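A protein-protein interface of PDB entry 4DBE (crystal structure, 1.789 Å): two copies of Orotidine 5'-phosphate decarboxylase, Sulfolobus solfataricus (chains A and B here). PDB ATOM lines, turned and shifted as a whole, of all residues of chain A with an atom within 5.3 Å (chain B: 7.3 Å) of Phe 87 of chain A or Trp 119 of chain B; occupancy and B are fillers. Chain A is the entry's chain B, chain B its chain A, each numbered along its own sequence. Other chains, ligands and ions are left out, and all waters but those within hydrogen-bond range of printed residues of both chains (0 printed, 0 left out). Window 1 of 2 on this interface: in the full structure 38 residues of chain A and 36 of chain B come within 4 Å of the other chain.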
ATOM      1  N   HIS A  85     -23.330   6.703 -31.186  1.00  0.00           N
ATOM      2  CA  HIS A  85     -22.874   7.374 -29.966  1.00  0.00           C
ATOM      3  C   HIS A  85     -23.658   8.641 -29.709  1.00  0.00           C
ATOM      4  O   HIS A  85     -24.048   9.347 -30.644  1.00  0.00           O
ATOM      5  CB  HIS A  85     -21.380   7.692 -30.019  1.00  0.00           C
ATOM      6  CG  HIS A  85     -20.509   6.541 -29.629  1.00  0.00           C
ATOM      7  ND1 HIS A  85     -20.288   6.186 -28.314  1.00  0.00           N
ATOM      8  CD2 HIS A  85     -19.804   5.662 -30.380  1.00  0.00           C
ATOM      9  CE1 HIS A  85     -19.478   5.143 -28.273  1.00  0.00           C
ATOM     10  NE2 HIS A  85     -19.163   4.809 -29.513  1.00  0.00           N
ATOM     11  N   SER A  86     -23.909   8.918 -28.438  1.00  0.00           N
ATOM     12  CA  SER A  86     -24.587  10.157 -28.085  1.00  0.00           C
ATOM     13  C   SER A  86     -23.593  11.305 -27.958  1.00  0.00           C
ATOM     14  O   SER A  86     -23.952  12.468 -28.142  1.00  0.00           O
ATOM     15  CB  SER A  86     -25.375   9.976 -26.787  1.00  0.00           C
ATOM     16  OG  SER A  86     -24.491   9.721 -25.719  1.00  0.00           O
ATOM     17  N   PHE A  87     -22.336  10.984 -27.674  1.00  0.00           N
ATOM     18  CA  PHE A  87     -21.351  12.034 -27.421  1.00  0.00           C
ATOM     19  C   PHE A  87     -21.206  13.040 -28.560  1.00  0.00           C
ATOM     20  O   PHE A  87     -20.979  14.227 -28.321  1.00  0.00           O
ATOM     21  CB  PHE A  87     -19.977  11.444 -27.094  1.00  0.00           C
ATOM     22  CG  PHE A  87     -19.014  12.455 -26.541  1.00  0.00           C
ATOM     23  CD1 PHE A  87     -19.010  12.762 -25.183  1.00  0.00           C
ATOM     24  CD2 PHE A  87     -18.125  13.114 -27.370  1.00  0.00           C
ATOM     25  CE1 PHE A  87     -18.126  13.694 -24.673  1.00  0.00           C
ATOM     26  CE2 PHE A  87     -17.240  14.056 -26.867  1.00  0.00           C
ATOM     27  CZ  PHE A  87     -17.243  14.348 -25.516  1.00  0.00           C
ATOM     28  N   ILE A  88     -21.328  12.561 -29.795  1.00  0.00           N
ATOM     29  CA  ILE A  88     -21.074  13.392 -30.965  1.00  0.00           C
ATOM     30  C   ILE A  88     -22.022  14.600 -31.077  1.00  0.00           C
ATOM     31  O   ILE A  88     -21.771  15.515 -31.848  1.00  0.00           O
ATOM     32  CB  ILE A  88     -21.130  12.556 -32.269  1.00  0.00           C
ATOM     33  CG1 ILE A  88     -22.537  11.989 -32.472  1.00  0.00           C
ATOM     34  CG2 ILE A  88     -20.097  11.431 -32.214  1.00  0.00           C
ATOM     35  CD1 ILE A  88     -22.640  10.969 -33.620  1.00  0.00           C
ATOM     36  N   GLY A  89     -23.117  14.585 -30.328  1.00  0.00           N
ATOM     37  CA  GLY A  89     -24.028  15.713 -30.312  1.00  0.00           C
ATOM     38  C   GLY A  89     -25.076  15.728 -31.412  1.00  0.00           C
ATOM     39  O   GLY A  89     -25.120  14.851 -32.288  1.00  0.00           O
ATOM     40  N   LYS A  91     -26.860  18.762 -33.574  1.00  0.00           N
ATOM     41  CA  LYS A  91     -26.890  19.501 -34.838  1.00  0.00           C
ATOM     42  C   LYS A  91     -25.821  19.081 -35.844  1.00  0.00           C
ATOM     43  O   LYS A  91     -24.626  19.233 -35.595  1.00  0.00           O
ATOM     44  CB  LYS A  91     -26.762  21.008 -34.590  1.00  0.00           C
ATOM     45  CG  LYS A  91     -28.079  21.763 -34.501  1.00  0.00           C
ATOM     46  CD  LYS A  91     -28.680  21.694 -33.106  1.00  0.00           C
ATOM     47  CE  LYS A  91     -29.859  22.655 -32.970  1.00  0.00           C
ATOM     48  NZ  LYS A  91     -30.538  22.514 -31.651  1.00  0.00           N
ATOM     49  N   VAL A 111     -25.509   5.154 -27.409  1.00  0.00           N
ATOM     50  CA  VAL A 111     -24.592   4.708 -26.361  1.00  0.00           C
ATOM     51  C   VAL A 111     -24.594   5.761 -25.241  1.00  0.00           C
ATOM     52  O   VAL A 111     -24.189   6.903 -25.452  1.00  0.00           O
ATOM     53  CB  VAL A 111     -23.145   4.537 -26.896  1.00  0.00           C
ATOM     54  CG1 VAL A 111     -22.183   4.162 -25.768  1.00  0.00           C
ATOM     55  CG2 VAL A 111     -23.085   3.522 -28.020  1.00  0.00           C
ATOM     56  N   TRP A 119     -14.331   4.771 -19.400  1.00  0.00           N
ATOM     57  CA  TRP A 119     -15.463   5.638 -19.731  1.00  0.00           C
ATOM     58  C   TRP A 119     -15.689   6.671 -18.640  1.00  0.00           C
ATOM     59  O   TRP A 119     -15.934   6.316 -17.487  1.00  0.00           O
ATOM     60  CB  TRP A 119     -16.734   4.817 -19.919  1.00  0.00           C
ATOM     61  CG  TRP A 119     -17.932   5.625 -20.314  1.00  0.00           C
ATOM     62  CD1 TRP A 119     -18.999   5.947 -19.530  1.00  0.00           C
ATOM     63  CD2 TRP A 119     -18.195   6.194 -21.605  1.00  0.00           C
ATOM     64  NE1 TRP A 119     -19.906   6.694 -20.246  1.00  0.00           N
ATOM     65  CE2 TRP A 119     -19.437   6.857 -21.524  1.00  0.00           C
ATOM     66  CE3 TRP A 119     -17.499   6.208 -22.821  1.00  0.00           C
ATOM     67  CZ2 TRP A 119     -20.000   7.534 -22.612  1.00  0.00           C
ATOM     68  CZ3 TRP A 119     -18.065   6.878 -23.906  1.00  0.00           C
ATOM     69  CH2 TRP A 119     -19.300   7.527 -23.792  1.00  0.00           C
ATOM     70  N   PHE A 123     -19.118  13.355 -18.634  1.00  0.00           N
ATOM     71  CA  PHE A 123     -20.150  13.841 -19.550  1.00  0.00           C
ATOM     72  C   PHE A 123     -21.578  13.370 -19.276  1.00  0.00           C
ATOM     73  O   PHE A 123     -22.477  13.625 -20.081  1.00  0.00           O
ATOM     74  CB  PHE A 123     -19.802  13.657 -21.041  1.00  0.00           C
ATOM     75  CG  PHE A 123     -18.638  12.739 -21.325  1.00  0.00           C
ATOM     76  CD1 PHE A 123     -18.852  11.401 -21.616  1.00  0.00           C
ATOM     77  CD2 PHE A 123     -17.341  13.234 -21.383  1.00  0.00           C
ATOM     78  CE1 PHE A 123     -17.793  10.565 -21.922  1.00  0.00           C
ATOM     79  CE2 PHE A 123     -16.274  12.401 -21.688  1.00  0.00           C
ATOM     80  CZ  PHE A 123     -16.505  11.062 -21.964  1.00  0.00           C
ATOM     81  N   TYR A 126     -24.352  15.958 -19.977  1.00  0.00           N
ATOM     82  CA  TYR A 126     -24.398  16.324 -21.385  1.00  0.00           C
ATOM     83  C   TYR A 126     -25.063  15.200 -22.183  1.00  0.00           C
ATOM     84  O   TYR A 126     -25.958  15.450 -22.991  1.00  0.00           O
ATOM     85  CB  TYR A 126     -22.984  16.596 -21.896  1.00  0.00           C
ATOM     86  CG  TYR A 126     -22.860  16.621 -23.406  1.00  0.00           C
ATOM     87  CD1 TYR A 126     -23.471  17.614 -24.157  1.00  0.00           C
ATOM     88  CD2 TYR A 126     -22.113  15.655 -24.076  1.00  0.00           C
ATOM     89  CE1 TYR A 126     -23.355  17.644 -25.543  1.00  0.00           C
ATOM     90  CE2 TYR A 126     -21.988  15.673 -25.459  1.00  0.00           C
ATOM     91  CZ  TYR A 126     -22.612  16.671 -26.188  1.00  0.00           C
ATOM     92  OH  TYR A 126     -22.486  16.696 -27.563  1.00  0.00           O
ATOM     93  N   ILE A 127     -24.636  13.965 -21.923  1.00  0.00           N
ATOM     94  CA  ILE A 127     -25.201  12.793 -22.598  1.00  0.00           C
ATOM     95  C   ILE A 127     -26.702  12.702 -22.358  1.00  0.00           C
ATOM     96  O   ILE A 127     -27.473  12.525 -23.292  1.00  0.00           O
ATOM     97  CB  ILE A 127     -24.548  11.472 -22.125  1.00  0.00           C
ATOM     98  CG1 ILE A 127     -23.053  11.446 -22.444  1.00  0.00           C
ATOM     99  CG2 ILE A 127     -25.260  10.267 -22.733  1.00  0.00           C
ATOM    100  CD1 ILE A 127     -22.727  11.824 -23.855  1.00  0.00           C
ATOM    101  N   HIS B  85     -11.965   7.715 -31.989  1.00  0.00           N
ATOM    102  CA  HIS B  85     -12.409   8.798 -31.128  1.00  0.00           C
ATOM    103  C   HIS B  85     -11.578   8.863 -29.858  1.00  0.00           C
ATOM    104  O   HIS B  85     -11.064   7.843 -29.387  1.00  0.00           O
ATOM    105  CB  HIS B  85     -13.875   8.610 -30.801  1.00  0.00           C
ATOM    106  CG  HIS B  85     -14.783   9.181 -31.834  1.00  0.00           C
ATOM    107  ND1 HIS B  85     -14.974  10.538 -31.978  1.00  0.00           N
ATOM    108  CD2 HIS B  85     -15.526   8.588 -32.799  1.00  0.00           C
ATOM    109  CE1 HIS B  85     -15.809  10.757 -32.978  1.00  0.00           C
ATOM    110  NE2 HIS B  85     -16.168   9.591 -33.486  1.00  0.00           N
ATOM    111  N   SER B  86     -11.434  10.071 -29.314  1.00  0.00           N
ATOM    112  CA  SER B  86     -10.772  10.249 -28.026  1.00  0.00           C
ATOM    113  C   SER B  86     -11.763  10.146 -26.861  1.00  0.00           C
ATOM    114  O   SER B  86     -11.386   9.748 -25.758  1.00  0.00           O
ATOM    115  CB  SER B  86     -10.046  11.601 -27.985  1.00  0.00           C
ATOM    116  OG  SER B  86     -10.974  12.656 -28.087  1.00  0.00           O
ATOM    117  N   PHE B  87     -13.031  10.485 -27.095  1.00  0.00           N
ATOM    118  CA  PHE B  87     -13.975  10.606 -25.981  1.00  0.00           C
ATOM    119  C   PHE B  87     -14.199   9.304 -25.211  1.00  0.00           C
ATOM    120  O   PHE B  87     -14.540   9.335 -24.017  1.00  0.00           O
ATOM    121  CB  PHE B  87     -15.307  11.228 -26.418  1.00  0.00           C
ATOM    122  CG  PHE B  87     -16.194  10.296 -27.203  1.00  0.00           C
ATOM    123  CD1 PHE B  87     -17.077   9.452 -26.554  1.00  0.00           C
ATOM    124  CD2 PHE B  87     -16.161  10.288 -28.587  1.00  0.00           C
ATOM    125  CE1 PHE B  87     -17.901   8.589 -27.271  1.00  0.00           C
ATOM    126  CE2 PHE B  87     -16.989   9.431 -29.322  1.00  0.00           C
ATOM    127  CZ  PHE B  87     -17.852   8.583 -28.668  1.00  0.00           C
ATOM    128  N   ILE B  88     -13.984   8.170 -25.882  1.00  0.00           N
ATOM    129  CA  ILE B  88     -14.165   6.860 -25.257  1.00  0.00           C
ATOM    130  C   ILE B  88     -13.176   6.562 -24.125  1.00  0.00           C
ATOM    131  O   ILE B  88     -13.409   5.663 -23.324  1.00  0.00           O
ATOM    132  CB  ILE B  88     -14.114   5.720 -26.300  1.00  0.00           C
ATOM    133  CG1 ILE B  88     -12.722   5.641 -26.930  1.00  0.00           C
ATOM    134  CG2 ILE B  88     -15.207   5.930 -27.353  1.00  0.00           C
ATOM    135  CD1 ILE B  88     -12.632   4.662 -28.109  1.00  0.00           C
ATOM    136  N   VAL B 111      -9.707  11.673 -32.849  1.00  0.00           N
ATOM    137  CA  VAL B 111     -10.652  12.757 -33.083  1.00  0.00           C
ATOM    138  C   VAL B 111     -10.700  13.676 -31.863  1.00  0.00           C
ATOM    139  O   VAL B 111     -11.138  13.269 -30.787  1.00  0.00           O
ATOM    140  CB  VAL B 111     -12.064  12.246 -33.376  1.00  0.00           C
ATOM    141  CG1 VAL B 111     -13.039  13.445 -33.516  1.00  0.00           C
ATOM    142  CG2 VAL B 111     -12.059  11.381 -34.632  1.00  0.00           C
ATOM    143  N   ALA B 112     -10.268  14.916 -32.055  1.00  0.00           N
ATOM    144  CA  ALA B 112     -10.215  15.918 -30.978  1.00  0.00           C
ATOM    145  C   ALA B 112     -11.418  16.860 -30.978  1.00  0.00           C
ATOM    146  O   ALA B 112     -12.088  17.029 -29.963  1.00  0.00           O
ATOM    147  CB  ALA B 112      -8.934  16.724 -31.091  1.00  0.00           C
ATOM    148  N   VAL B 113     -11.679  17.492 -32.118  1.00  0.00           N
ATOM    149  CA  VAL B 113     -12.805  18.409 -32.236  1.00  0.00           C
ATOM    150  C   VAL B 113     -13.469  18.141 -33.583  1.00  0.00           C
ATOM    151  O   VAL B 113     -12.804  18.188 -34.616  1.00  0.00           O
ATOM    152  CB  VAL B 113     -12.336  19.863 -32.207  1.00  0.00           C
ATOM    153  CG1 VAL B 113     -13.542  20.825 -32.337  1.00  0.00           C
ATOM    154  CG2 VAL B 113     -11.511  20.139 -30.941  1.00  0.00           C
ATOM    155  N   MET B 114     -14.766  17.855 -33.586  1.00  0.00           N
ATOM    156  CA  MET B 114     -15.421  17.563 -34.858  1.00  0.00           C
ATOM    157  C   MET B 114     -15.901  18.816 -35.594  1.00  0.00           C
ATOM    158  O   MET B 114     -15.885  19.933 -35.041  1.00  0.00           O
ATOM    159  CB  MET B 114     -16.534  16.522 -34.689  1.00  0.00           C
ATOM    160  CG  MET B 114     -15.985  15.127 -34.389  1.00  0.00           C
ATOM    161  SD  MET B 114     -17.276  13.880 -34.391  1.00  0.00           S
ATOM    162  CE  MET B 114     -17.660  13.790 -36.146  1.00  0.00           C
ATOM    163  N   SER B 115     -16.308  18.634 -36.850  1.00  0.00           N
ATOM    164  CA  SER B 115     -16.592  19.777 -37.722  1.00  0.00           C
ATOM    165  C   SER B 115     -18.027  20.289 -37.651  1.00  0.00           C
ATOM    166  O   SER B 115     -18.298  21.433 -38.013  1.00  0.00           O
ATOM    167  CB  SER B 115     -16.214  19.452 -39.176  1.00  0.00           C
ATOM    168  OG  SER B 115     -16.980  18.357 -39.661  1.00  0.00           O
ATOM    169  N   HIS B 116     -18.952  19.456 -37.195  1.00  0.00           N
ATOM    170  CA  HIS B 116     -20.354  19.851 -37.159  1.00  0.00           C
ATOM    171  C   HIS B 116     -20.680  20.769 -35.960  1.00  0.00           C
ATOM    172  O   HIS B 116     -19.985  20.766 -34.938  1.00  0.00           O
ATOM    173  CB  HIS B 116     -21.285  18.623 -37.195  1.00  0.00           C
ATOM    174  CG  HIS B 116     -21.133  17.714 -36.013  1.00  0.00           C
ATOM    175  ND1 HIS B 116     -20.040  16.890 -35.839  1.00  0.00           N
ATOM    176  CD2 HIS B 116     -21.936  17.501 -34.947  1.00  0.00           C
ATOM    177  CE1 HIS B 116     -20.173  16.217 -34.710  1.00  0.00           C
ATOM    178  NE2 HIS B 116     -21.315  16.570 -34.149  1.00  0.00           N
ATOM    179  N   GLU B 117     -21.740  21.550 -36.112  1.00  0.00           N
ATOM    180  CA  GLU B 117     -22.114  22.558 -35.129  1.00  0.00           C
ATOM    181  C   GLU B 117     -22.465  21.950 -33.772  1.00  0.00           C
ATOM    182  O   GLU B 117     -22.205  22.545 -32.725  1.00  0.00           O
ATOM    183  CB  GLU B 117     -23.283  23.390 -35.672  1.00  0.00           C
ATOM    184  CG  GLU B 117     -23.922  24.318 -34.656  1.00  0.00           C
ATOM    185  CD  GLU B 117     -25.133  25.045 -35.216  1.00  0.00           C
ATOM    186  OE1 GLU B 117     -25.190  25.250 -36.450  1.00  0.00           O
ATOM    187  OE2 GLU B 117     -26.030  25.400 -34.421  1.00  0.00           O
ATOM    188  N   GLY B 118     -23.026  20.748 -33.798  1.00  0.00           N
ATOM    189  CA  GLY B 118     -23.498  20.085 -32.595  1.00  0.00           C
ATOM    190  C   GLY B 118     -22.449  19.442 -31.708  1.00  0.00           C
ATOM    191  O   GLY B 118     -22.773  18.998 -30.613  1.00  0.00           O
ATOM    192  N   TRP B 119     -21.203  19.380 -32.172  1.00  0.00           N
ATOM    193  CA  TRP B 119     -20.102  18.888 -31.355  1.00  0.00           C
ATOM    194  C   TRP B 119     -19.879  19.782 -30.139  1.00  0.00           C
ATOM    195  O   TRP B 119     -19.850  21.001 -30.266  1.00  0.00           O
ATOM    196  CB  TRP B 119     -18.808  18.842 -32.172  1.00  0.00           C
ATOM    197  CG  TRP B 119     -17.624  18.376 -31.377  1.00  0.00           C
ATOM    198  CD1 TRP B 119     -16.663  19.153 -30.795  1.00  0.00           C
ATOM    199  CD2 TRP B 119     -17.282  17.020 -31.073  1.00  0.00           C
ATOM    200  NE1 TRP B 119     -15.740  18.364 -30.153  1.00  0.00           N
ATOM    201  CE2 TRP B 119     -16.096  17.050 -30.310  1.00  0.00           C
ATOM    202  CE3 TRP B 119     -17.858  15.785 -31.378  1.00  0.00           C
ATOM    203  CZ2 TRP B 119     -15.477  15.890 -29.844  1.00  0.00           C
ATOM    204  CZ3 TRP B 119     -17.243  14.633 -30.919  1.00  0.00           C
ATOM    205  CH2 TRP B 119     -16.065  14.692 -30.157  1.00  0.00           C
ATOM    206  N   SER B 120     -19.702  19.174 -28.973  1.00  0.00           N
ATOM    207  CA  SER B 120     -19.446  19.932 -27.747  1.00  0.00           C
ATOM    208  C   SER B 120     -17.955  20.052 -27.460  1.00  0.00           C
ATOM    209  O   SER B 120     -17.217  19.077 -27.557  1.00  0.00           O
ATOM    210  CB  SER B 120     -20.143  19.267 -26.555  1.00  0.00           C
ATOM    211  OG  SER B 120     -19.741  19.864 -25.330  1.00  0.00           O
ATOM    212  N   THR B 121     -17.509  21.249 -27.099  1.00  0.00           N
ATOM    213  CA  THR B 121     -16.126  21.437 -26.676  1.00  0.00           C
ATOM    214  C   THR B 121     -16.066  21.563 -25.158  1.00  0.00           C
ATOM    215  O   THR B 121     -15.085  22.042 -24.598  1.00  0.00           O
ATOM    216  CB  THR B 121     -15.465  22.654 -27.355  1.00  0.00           C
ATOM    217  OG1 THR B 121     -16.275  23.820 -27.149  1.00  0.00           O
ATOM    218  CG2 THR B 121     -15.299  22.397 -28.862  1.00  0.00           C
ATOM    219  N   LEU B 122     -17.129  21.107 -24.506  1.00  0.00           N
ATOM    220  CA  LEU B 122     -17.223  21.118 -23.051  1.00  0.00           C
ATOM    221  C   LEU B 122     -16.088  20.393 -22.340  1.00  0.00           C
ATOM    222  O   LEU B 122     -15.725  20.757 -21.221  1.00  0.00           O
ATOM    223  CB  LEU B 122     -18.547  20.497 -22.609  1.00  0.00           C
ATOM    224  CG  LEU B 122     -19.720  21.462 -22.494  1.00  0.00           C
ATOM    225  CD1 LEU B 122     -21.002  20.711 -22.173  1.00  0.00           C
ATOM    226  CD2 LEU B 122     -19.420  22.513 -21.431  1.00  0.00           C
ATOM    227  N   PHE B 123     -15.536  19.361 -22.970  1.00  0.00           N
ATOM    228  CA  PHE B 123     -14.602  18.489 -22.266  1.00  0.00           C
ATOM    229  C   PHE B 123     -13.202  18.495 -22.874  1.00  0.00           C
ATOM    230  O   PHE B 123     -12.568  17.452 -22.998  1.00  0.00           O
ATOM    231  CB  PHE B 123     -15.171  17.064 -22.195  1.00  0.00           C
ATOM    232  CG  PHE B 123     -16.594  17.012 -21.716  1.00  0.00           C
ATOM    233  CD1 PHE B 123     -16.883  16.989 -20.361  1.00  0.00           C
ATOM    234  CD2 PHE B 123     -17.643  17.005 -22.618  1.00  0.00           C
ATOM    235  CE1 PHE B 123     -18.202  16.948 -19.915  1.00  0.00           C
ATOM    236  CE2 PHE B 123     -18.961  16.968 -22.180  1.00  0.00           C
ATOM    237  CZ  PHE B 123     -19.239  16.939 -20.824  1.00  0.00           C
ATOM    238  N   TYR B 126     -10.411  17.033 -20.595  1.00  0.00           N
ATOM    239  CA  TYR B 126     -10.407  15.575 -20.549  1.00  0.00           C
ATOM    240  C   TYR B 126      -9.898  14.996 -21.869  1.00  0.00           C
ATOM    241  O   TYR B 126      -9.071  14.079 -21.893  1.00  0.00           O
ATOM    242  CB  TYR B 126     -11.806  15.038 -20.244  1.00  0.00           C
ATOM    243  CG  TYR B 126     -11.869  13.532 -20.283  1.00  0.00           C
ATOM    244  CD1 TYR B 126     -11.374  12.778 -19.231  1.00  0.00           C
ATOM    245  CD2 TYR B 126     -12.398  12.863 -21.379  1.00  0.00           C
ATOM    246  CE1 TYR B 126     -11.412  11.401 -19.259  1.00  0.00           C
ATOM    247  CE2 TYR B 126     -12.442  11.476 -21.419  1.00  0.00           C
ATOM    248  CZ  TYR B 126     -11.953  10.755 -20.350  1.00  0.00           C
ATOM    249  OH  TYR B 126     -11.985   9.385 -20.367  1.00  0.00           O
ATOM    250  N   ILE B 127     -10.389  15.553 -22.969  1.00  0.00           N
ATOM    251  CA  ILE B 127      -9.990  15.108 -24.298  1.00  0.00           C
ATOM    252  C   ILE B 127      -8.487  15.286 -24.478  1.00  0.00           C
ATOM    253  O   ILE B 127      -7.806  14.407 -24.986  1.00  0.00           O
ATOM    254  CB  ILE B 127     -10.770  15.878 -25.399  1.00  0.00           C
ATOM    255  CG1 ILE B 127     -12.255  15.526 -25.343  1.00  0.00           C
ATOM    256  CG2 ILE B 127     -10.202  15.604 -26.780  1.00  0.00           C
ATOM    257  CD1 ILE B 127     -12.539  14.034 -25.371  1.00  0.00           C
ATOM    258  N   LYS B 145     -13.546  24.860 -37.308  1.00  0.00           N
ATOM    259  CA  LYS B 145     -13.274  25.287 -35.938  1.00  0.00           C
ATOM    260  C   LYS B 145     -11.840  25.814 -35.848  1.00  0.00           C
ATOM    261  O   LYS B 145     -11.009  25.263 -35.128  1.00  0.00           O
ATOM    262  CB  LYS B 145     -13.446  24.104 -34.979  1.00  0.00           C
ATOM    263  CG  LYS B 145     -14.731  23.300 -35.171  1.00  0.00           C
ATOM    264  CD  LYS B 145     -15.957  24.125 -34.779  1.00  0.00           C
ATOM    265  CE  LYS B 145     -17.261  23.388 -35.108  1.00  0.00           C
ATOM    266  NZ  LYS B 145     -17.407  22.106 -34.359  1.00  0.00           N
ATOM    267  N   HIS B 148      -9.987  26.326 -32.568  1.00  0.00           N
ATOM    268  CA  HIS B 148      -9.575  25.066 -31.950  1.00  0.00           C
ATOM    269  C   HIS B 148      -8.322  24.514 -32.606  1.00  0.00           C
ATOM    270  O   HIS B 148      -7.464  23.974 -31.921  1.00  0.00           O
ATOM    271  CB  HIS B 148     -10.709  24.038 -31.923  1.00  0.00           C
ATOM    272  CG  HIS B 148     -11.820  24.414 -31.000  1.00  0.00           C
ATOM    273  ND1 HIS B 148     -12.826  25.284 -31.365  1.00  0.00           N
ATOM    274  CD2 HIS B 148     -12.058  24.083 -29.710  1.00  0.00           C
ATOM    275  CE1 HIS B 148     -13.651  25.451 -30.346  1.00  0.00           C
ATOM    276  NE2 HIS B 148     -13.205  24.737 -29.328  1.00  0.00           N
ATOM    277  N   TYR B 152      -5.101  23.709 -30.415  1.00  0.00           N
ATOM    278  CA  TYR B 152      -4.482  22.380 -30.382  1.00  0.00           C
ATOM    279  C   TYR B 152      -3.043  22.348 -30.875  1.00  0.00           C
ATOM    280  O   TYR B 152      -2.245  21.532 -30.398  1.00  0.00           O
ATOM    281  CB  TYR B 152      -5.335  21.315 -31.104  1.00  0.00           C
ATOM    282  CG  TYR B 152      -6.390  20.719 -30.199  1.00  0.00           C
ATOM    283  CD1 TYR B 152      -7.602  21.358 -30.007  1.00  0.00           C
ATOM    284  CD2 TYR B 152      -6.156  19.542 -29.499  1.00  0.00           C
ATOM    285  CE1 TYR B 152      -8.561  20.839 -29.162  1.00  0.00           C
ATOM    286  CE2 TYR B 152      -7.116  19.010 -28.649  1.00  0.00           C
ATOM    287  CZ  TYR B 152      -8.314  19.662 -28.487  1.00  0.00           C
ATOM    288  OH  TYR B 152      -9.283  19.143 -27.649  1.00  0.00           O
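NE2 of His 116 of chain B lies within hydrogen-bond range of O of Ile 88 of chain A (2.6 Å). N of Gly 118 of chain B sits at hydrogen-bond distance from O of Lys 91 of chain A, at 2.8 Å.
A ring nitrogen (NE2) of His 116 of chain B lies close to the backbone NH (N) of Trp 119 of chain B. The side-chain amino group (NZ) of Lys 145 of chain B lies within hydrogen-bond range of the backbone carbonyl oxygen (O) of His 116 of chain B, at 3.0 Å. N of Leu 122 of chain B sits at hydrogen-bond distance from OG of Ser 120 of chain B (3.0 Å). The backbone carbonyl oxygen of Phe 87 of chain A is in hydrogen-bond range of the side-chain hydroxyl of Tyr 126 of chain A (3.0 Å).
CZ of Phe 87 of chain B touches ND1 of His 85 of chain A (3.4 Å). Phe 87 of chain B touches Phe 87 of chain A (CG to CD2, 3.4 Å). Ile 88 of chain A touches Gly 118 of chain B (O to O, 3.8 Å). Lys 91 of chain A touches His 116 of chain B (O to CD2, 3.3 Å). CZ3 of Trp 119 of chain A touches CE1 of Phe 87 of chain B, at 3.8 Å. O of Phe 87 of chain B touches CZ of Phe 123 of chain A, 3.3 Å away. Phe 123 of chain B touches Phe 123 of chain A (CZ to CB, 3.3 Å). CD2 of Tyr 126 of chain B touches CE2 of Phe 123 of chain A, at 3.9 Å. Tyr 126 of chain A touches Gly 118 of chain B (OH to O, 3.8 Å). CZ of Tyr 126 of chain A touches CB of Ser 120 of chain B, 3.6 Å away.
Phe 87 of chain A touches just these residues of chain B: Phe 87, Trp 119 and Phe 123. Of the printed residues of chain A, Trp 119 of chain B touches Phe 87 (3.6 Å) and Ile 88 (3.8 Å). Printed residues of chain A within 4 Å of Phe 87 of chain B: His 85 (3.4 Å), Phe 87 (3.4 Å), Trp 119 (3.8 Å) and Phe 123 (3.3 Å). Printed residues of chain A within 4 Å of Glu 117 of chain B: Lys 91 (3.7 Å). Of the printed residues of chain B, Phe 123 of chain A touches Phe 87 (3.3 Å), Phe 123 (3.3 Å) and Tyr 126 (3.9 Å). Of the printed residues of chain B, Trp 119 of chain A touches Phe 87 (3.8 Å). Of the printed residues of chain B, Ile 88 of chain A touches His 116, Gly 118 and Trp 119. The nearest residue of chain B that does not touch Phe 87 of chain A is Ile 127 of chain B (4.7 Å). The nearest residue of chain A that does not touch Trp 119 of chain B is Tyr 126 of chain A (4.8 Å).
Hydrophobic or aromatic side chains of chain B that line the printed part of chain A: Phe 87, His 116, Trp 119, Phe 123 and Tyr 126. Of the 11 printed residues of chain A, 8 touch a printed residue of chain B. Printed residues of chain A that touch a printed residue of chain B: His 85, Phe 87, Ile 88, Gly 89, Lys 91, Trp 119, Phe 123 and Tyr 126. Hydrophobic or aromatic side chains of chain A within 4 Å of the printed part of chain B: His 85, Phe 87, Trp 119, Phe 123 and Tyr 126. Among the printed residues, 18 pairs touch across the chains. Among the printed residues, no Asp or Glu carboxylate lies within 4 Å of a Lys or Arg side-chain nitrogen of the other chain.
His 85 of chain A touches Phe 87 of chain B, but with the chains exchanged Phe 87 of chain A does not touch His 85 of chain B (6.1 Å). Phe 87 of chain A touches its own counterpart, Phe 87 of chain B. Phe 87 of chain A touches Trp 119 of chain B, and with the chains exchanged Trp 119 of chain A touches Phe 87 of chain B. Phe 123 of chain A touches Tyr 126 of chain B, and with the chains exchanged Tyr 126 of chain A touches Phe 123 of chain B. Positions printed for both chains: 85, 86, 87, 88, 111, 119, 123, 126 and 127. Of the 18 pairs that touch across the chains among the printed residues, 8 have their exchanged pair printed and touching as well.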
